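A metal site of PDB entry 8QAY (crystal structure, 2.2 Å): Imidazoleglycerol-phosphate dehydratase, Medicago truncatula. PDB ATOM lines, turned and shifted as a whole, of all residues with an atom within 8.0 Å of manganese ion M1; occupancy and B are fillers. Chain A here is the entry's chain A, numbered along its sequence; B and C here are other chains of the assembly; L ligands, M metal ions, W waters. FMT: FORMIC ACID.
The side-chain hydroxyl of Ser 148 sits at hydrogen-bond distance from a ring nitrogen (ND1) of His 144 (3.1 Å).
OD1 of Asn 166 of chain B is in hydrogen-bond range of N of His 169 of chain B (3.0 Å).
ND1 of His 169 of chain B sits at hydrogen-bond distance from OE1 of Glu 108 of chain B, at 2.7 Å.
Manganese ion M1 is bound by OE1 of Glu 76, O2 of the ligand, NE2 of His 72, water W1, NE2 of His 144 and NE2 of His 169 of chain B.
Manganese ion M1 has six donor atoms within binding distance.
Water W1 lies within hydrogen-bond range of the side-chain carboxylate of Asp 107 of chain B, the side-chain carboxylate of Glu 76 and the guanidinium group of Arg 120 of chain C.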
ATOM      1  N   HIS A  72      -3.767  21.120   8.243  1.00  0.00           N
ATOM      2  CA  HIS A  72      -3.706  21.562   6.851  1.00  0.00           C
ATOM      3  C   HIS A  72      -3.956  23.058   6.695  1.00  0.00           C
ATOM      4  O   HIS A  72      -3.192  23.762   6.027  1.00  0.00           O
ATOM      5  CB  HIS A  72      -4.733  20.756   6.049  1.00  0.00           C
ATOM      6  CG  HIS A  72      -4.670  20.973   4.572  1.00  0.00           C
ATOM      7  ND1 HIS A  72      -4.429  19.940   3.687  1.00  0.00           N
ATOM      8  CD2 HIS A  72      -4.870  22.081   3.821  1.00  0.00           C
ATOM      9  CE1 HIS A  72      -4.465  20.404   2.445  1.00  0.00           C
ATOM     10  NE2 HIS A  72      -4.739  21.699   2.499  1.00  0.00           N
ATOM     11  N   HIS A  73      -5.055  23.565   7.272  1.00  0.00           N
ATOM     12  CA  HIS A  73      -5.378  24.971   7.078  1.00  0.00           C
ATOM     13  C   HIS A  73      -4.309  25.877   7.689  1.00  0.00           C
ATOM     14  O   HIS A  73      -3.857  26.845   7.045  1.00  0.00           O
ATOM     15  CB  HIS A  73      -6.753  25.265   7.668  1.00  0.00           C
ATOM     16  CG  HIS A  73      -7.862  24.484   7.030  1.00  0.00           C
ATOM     17  ND1 HIS A  73      -9.038  24.190   7.682  1.00  0.00           N
ATOM     18  CD2 HIS A  73      -7.982  23.966   5.778  1.00  0.00           C
ATOM     19  CE1 HIS A  73      -9.827  23.511   6.869  1.00  0.00           C
ATOM     20  NE2 HIS A  73      -9.208  23.365   5.718  1.00  0.00           N
ATOM     21  N   ASN A  75      -1.130  25.067   8.246  1.00  0.00           N
ATOM     22  CA  ASN A  75       0.068  24.886   7.422  1.00  0.00           C
ATOM     23  C   ASN A  75      -0.039  25.714   6.143  1.00  0.00           C
ATOM     24  O   ASN A  75       0.881  26.475   5.805  1.00  0.00           O
ATOM     25  CB  ASN A  75       0.257  23.396   7.129  1.00  0.00           C
ATOM     26  CG  ASN A  75       1.559  23.093   6.381  1.00  0.00           C
ATOM     27  OD1 ASN A  75       2.644  23.057   6.976  1.00  0.00           O
ATOM     28  ND2 ASN A  75       1.441  22.825   5.082  1.00  0.00           N
ATOM     29  N   GLU A  76      -1.172  25.622   5.459  1.00  0.00           N
ATOM     30  CA  GLU A  76      -1.352  26.354   4.209  1.00  0.00           C
ATOM     31  C   GLU A  76      -1.308  27.860   4.452  1.00  0.00           C
ATOM     32  O   GLU A  76      -0.596  28.599   3.749  1.00  0.00           O
ATOM     33  CB  GLU A  76      -2.672  25.937   3.543  1.00  0.00           C
ATOM     34  CG  GLU A  76      -2.990  26.699   2.262  1.00  0.00           C
ATOM     35  CD  GLU A  76      -4.039  25.997   1.398  1.00  0.00           C
ATOM     36  OE1 GLU A  76      -4.542  24.935   1.825  1.00  0.00           O
ATOM     37  OE2 GLU A  76      -4.339  26.503   0.286  1.00  0.00           O
ATOM     38  N   ASP A  77      -2.048  28.348   5.441  1.00  0.00           N
ATOM     39  CA  ASP A  77      -2.157  29.788   5.621  1.00  0.00           C
ATOM     40  C   ASP A  77      -0.850  30.403   6.115  1.00  0.00           C
ATOM     41  O   ASP A  77      -0.519  31.546   5.749  1.00  0.00           O
ATOM     42  CB  ASP A  77      -3.315  30.104   6.562  1.00  0.00           C
ATOM     43  CG  ASP A  77      -4.672  29.823   5.904  1.00  0.00           C
ATOM     44  OD1 ASP A  77      -4.720  29.630   4.675  1.00  0.00           O
ATOM     45  OD2 ASP A  77      -5.693  29.791   6.607  1.00  0.00           O
ATOM     46  N   LEU A  80       1.308  30.633   2.841  1.00  0.00           N
ATOM     47  CA  LEU A  80       0.821  31.753   2.036  1.00  0.00           C
ATOM     48  C   LEU A  80       1.280  33.091   2.593  1.00  0.00           C
ATOM     49  O   LEU A  80       1.759  33.951   1.862  1.00  0.00           O
ATOM     50  CB  LEU A  80      -0.705  31.720   1.958  1.00  0.00           C
ATOM     51  CG  LEU A  80      -1.403  30.591   1.202  1.00  0.00           C
ATOM     52  CD1 LEU A  80      -2.902  30.633   1.460  1.00  0.00           C
ATOM     53  CD2 LEU A  80      -1.134  30.711  -0.309  1.00  0.00           C
ATOM     54  N   LEU A 141       2.057  17.642   4.198  1.00  0.00           N
ATOM     55  CA  LEU A 141       2.001  19.091   4.322  1.00  0.00           C
ATOM     56  C   LEU A 141       3.304  19.760   3.901  1.00  0.00           C
ATOM     57  O   LEU A 141       3.322  20.980   3.716  1.00  0.00           O
ATOM     58  CB  LEU A 141       1.668  19.481   5.763  1.00  0.00           C
ATOM     59  CG  LEU A 141       0.318  18.963   6.233  1.00  0.00           C
ATOM     60  CD1 LEU A 141       0.077  19.415   7.664  1.00  0.00           C
ATOM     61  CD2 LEU A 141      -0.808  19.433   5.298  1.00  0.00           C
ATOM     62  N   HIS A 144       2.815  20.911   0.321  1.00  0.00           N
ATOM     63  CA  HIS A 144       1.829  21.978   0.331  1.00  0.00           C
ATOM     64  C   HIS A 144       2.391  23.263   0.921  1.00  0.00           C
ATOM     65  O   HIS A 144       1.972  24.350   0.524  1.00  0.00           O
ATOM     66  CB  HIS A 144       0.588  21.535   1.109  1.00  0.00           C
ATOM     67  CG  HIS A 144      -0.657  22.285   0.748  1.00  0.00           C
ATOM     68  ND1 HIS A 144      -0.653  23.627   0.446  1.00  0.00           N
ATOM     69  CD2 HIS A 144      -1.955  21.888   0.668  1.00  0.00           C
ATOM     70  CE1 HIS A 144      -1.882  24.026   0.182  1.00  0.00           C
ATOM     71  NE2 HIS A 144      -2.692  22.993   0.299  1.00  0.00           N
ATOM     72  N   SER A 148       2.406  26.521  -1.519  1.00  0.00           N
ATOM     73  CA  SER A 148       1.698  27.731  -1.122  1.00  0.00           C
ATOM     74  C   SER A 148       2.655  28.919  -1.023  1.00  0.00           C
ATOM     75  O   SER A 148       2.307  30.035  -1.414  1.00  0.00           O
ATOM     76  CB  SER A 148       0.977  27.543   0.208  1.00  0.00           C
ATOM     77  OG  SER A 148      -0.111  26.651   0.088  1.00  0.00           O
ATOM     78  N   LEU B 106     -10.038  20.740  -6.507  1.00  0.00           N
ATOM     79  CA  LEU B 106      -9.469  21.413  -5.347  1.00  0.00           C
ATOM     80  C   LEU B 106      -7.954  21.333  -5.529  1.00  0.00           C
ATOM     81  O   LEU B 106      -7.348  20.302  -5.222  1.00  0.00           O
ATOM     82  CB  LEU B 106      -9.896  20.770  -4.033  1.00  0.00           C
ATOM     83  CG  LEU B 106      -9.826  21.682  -2.800  1.00  0.00           C
ATOM     84  CD1 LEU B 106     -10.254  20.880  -1.580  1.00  0.00           C
ATOM     85  CD2 LEU B 106      -8.443  22.304  -2.574  1.00  0.00           C
ATOM     86  N   ASP B 107      -7.368  22.427  -6.023  1.00  0.00           N
ATOM     87  CA  ASP B 107      -5.961  22.456  -6.393  1.00  0.00           C
ATOM     88  C   ASP B 107      -5.652  21.274  -7.303  1.00  0.00           C
ATOM     89  O   ASP B 107      -6.270  21.145  -8.367  1.00  0.00           O
ATOM     90  CB  ASP B 107      -5.073  22.485  -5.137  1.00  0.00           C
ATOM     91  CG  ASP B 107      -5.196  23.799  -4.346  1.00  0.00           C
ATOM     92  OD1 ASP B 107      -5.907  24.732  -4.801  1.00  0.00           O
ATOM     93  OD2 ASP B 107      -4.577  23.912  -3.274  1.00  0.00           O
ATOM     94  N   GLU B 108      -4.725  20.404  -6.915  1.00  0.00           N
ATOM     95  CA  GLU B 108      -4.321  19.301  -7.788  1.00  0.00           C
ATOM     96  C   GLU B 108      -5.348  18.188  -7.841  1.00  0.00           C
ATOM     97  O   GLU B 108      -5.263  17.340  -8.733  1.00  0.00           O
ATOM     98  CB  GLU B 108      -2.952  18.743  -7.350  1.00  0.00           C
ATOM     99  CG  GLU B 108      -3.017  17.506  -6.398  1.00  0.00           C
ATOM    100  CD  GLU B 108      -3.646  17.774  -5.031  1.00  0.00           C
ATOM    101  OE1 GLU B 108      -3.724  18.957  -4.608  1.00  0.00           O
ATOM    102  OE2 GLU B 108      -4.065  16.806  -4.369  1.00  0.00           O
ATOM    103  N   ASN B 166      -3.113  15.041  -2.476  1.00  0.00           N
ATOM    104  CA  ASN B 166      -3.292  15.359  -1.052  1.00  0.00           C
ATOM    105  C   ASN B 166      -4.602  14.774  -0.579  1.00  0.00           C
ATOM    106  O   ASN B 166      -5.649  15.012  -1.179  1.00  0.00           O
ATOM    107  CB  ASN B 166      -3.256  16.867  -0.827  1.00  0.00           C
ATOM    108  CG  ASN B 166      -3.388  17.250   0.653  1.00  0.00           C
ATOM    109  OD1 ASN B 166      -4.490  17.269   1.191  1.00  0.00           O
ATOM    110  ND2 ASN B 166      -2.254  17.511   1.300  1.00  0.00           N
ATOM    111  N   HIS B 168      -6.528  15.269   2.090  1.00  0.00           N
ATOM    112  CA  HIS B 168      -7.512  16.278   2.445  1.00  0.00           C
ATOM    113  C   HIS B 168      -8.149  16.892   1.196  1.00  0.00           C
ATOM    114  O   HIS B 168      -9.367  17.071   1.124  1.00  0.00           O
ATOM    115  CB  HIS B 168      -6.816  17.332   3.334  1.00  0.00           C
ATOM    116  CG  HIS B 168      -7.700  18.377   3.962  1.00  0.00           C
ATOM    117  ND1 HIS B 168      -7.466  18.856   5.233  1.00  0.00           N
ATOM    118  CD2 HIS B 168      -8.736  19.105   3.466  1.00  0.00           C
ATOM    119  CE1 HIS B 168      -8.358  19.801   5.523  1.00  0.00           C
ATOM    120  NE2 HIS B 168      -9.134  19.965   4.461  1.00  0.00           N
ATOM    121  N   HIS B 169      -7.335  17.195   0.179  1.00  0.00           N
ATOM    122  CA  HIS B 169      -7.870  17.766  -1.058  1.00  0.00           C
ATOM    123  C   HIS B 169      -8.835  16.808  -1.749  1.00  0.00           C
ATOM    124  O   HIS B 169      -9.927  17.206  -2.154  1.00  0.00           O
ATOM    125  CB  HIS B 169      -6.721  18.119  -2.011  1.00  0.00           C
ATOM    126  CG  HIS B 169      -5.971  19.346  -1.619  1.00  0.00           C
ATOM    127  ND1 HIS B 169      -4.863  19.801  -2.300  1.00  0.00           N
ATOM    128  CD2 HIS B 169      -6.197  20.252  -0.629  1.00  0.00           C
ATOM    129  CE1 HIS B 169      -4.445  20.916  -1.751  1.00  0.00           C
ATOM    130  NE2 HIS B 169      -5.238  21.226  -0.747  1.00  0.00           N
ATOM    131  N   GLU B 172     -12.105  16.444   0.333  1.00  0.00           N
ATOM    132  CA  GLU B 172     -12.900  17.664   0.292  1.00  0.00           C
ATOM    133  C   GLU B 172     -13.480  17.902  -1.106  1.00  0.00           C
ATOM    134  O   GLU B 172     -14.648  18.265  -1.236  1.00  0.00           O
ATOM    135  CB  GLU B 172     -12.065  18.847   0.759  1.00  0.00           C
ATOM    136  CG  GLU B 172     -12.890  20.090   1.037  1.00  0.00           C
ATOM    137  CD  GLU B 172     -12.067  21.223   1.624  1.00  0.00           C
ATOM    138  OE1 GLU B 172     -11.244  20.961   2.524  1.00  0.00           O
ATOM    139  OE2 GLU B 172     -12.250  22.380   1.197  1.00  0.00           O
ATOM    140  N   ARG C 120      -6.068  30.501  -5.835  1.00  0.00           N
ATOM    141  CA  ARG C 120      -4.864  29.680  -5.758  1.00  0.00           C
ATOM    142  C   ARG C 120      -4.511  29.165  -7.151  1.00  0.00           C
ATOM    143  O   ARG C 120      -5.296  28.418  -7.755  1.00  0.00           O
ATOM    144  CB  ARG C 120      -5.090  28.497  -4.811  1.00  0.00           C
ATOM    145  CG  ARG C 120      -5.339  28.906  -3.350  1.00  0.00           C
ATOM    146  CD  ARG C 120      -5.585  27.689  -2.466  1.00  0.00           C
ATOM    147  NE  ARG C 120      -6.687  26.859  -2.959  1.00  0.00           N
ATOM    148  CZ  ARG C 120      -7.964  27.055  -2.655  1.00  0.00           C
ATOM    149  NH1 ARG C 120      -8.347  28.045  -1.868  1.00  0.00           N
ATOM    150  NH2 ARG C 120      -8.887  26.250  -3.182  1.00  0.00           N
HETATM  151  C   FMT L   1      -7.892  22.339   2.100  1.00  0.00           C
HETATM  152  O1  FMT L   1      -8.968  22.783   2.600  1.00  0.00           O
HETATM  153  O2  FMT L   1      -7.098  23.112   1.487  1.00  0.00           O
HETATM  154 MN    MN M   1      -4.997  23.090   0.730  1.00  0.00          MN
HETATM  155 MN    MN M   2     -10.272  21.971   4.147  1.00  0.00          MN
HETATM  156  O   HOH W   1      -5.798  24.445  -0.949  1.00  0.00           O
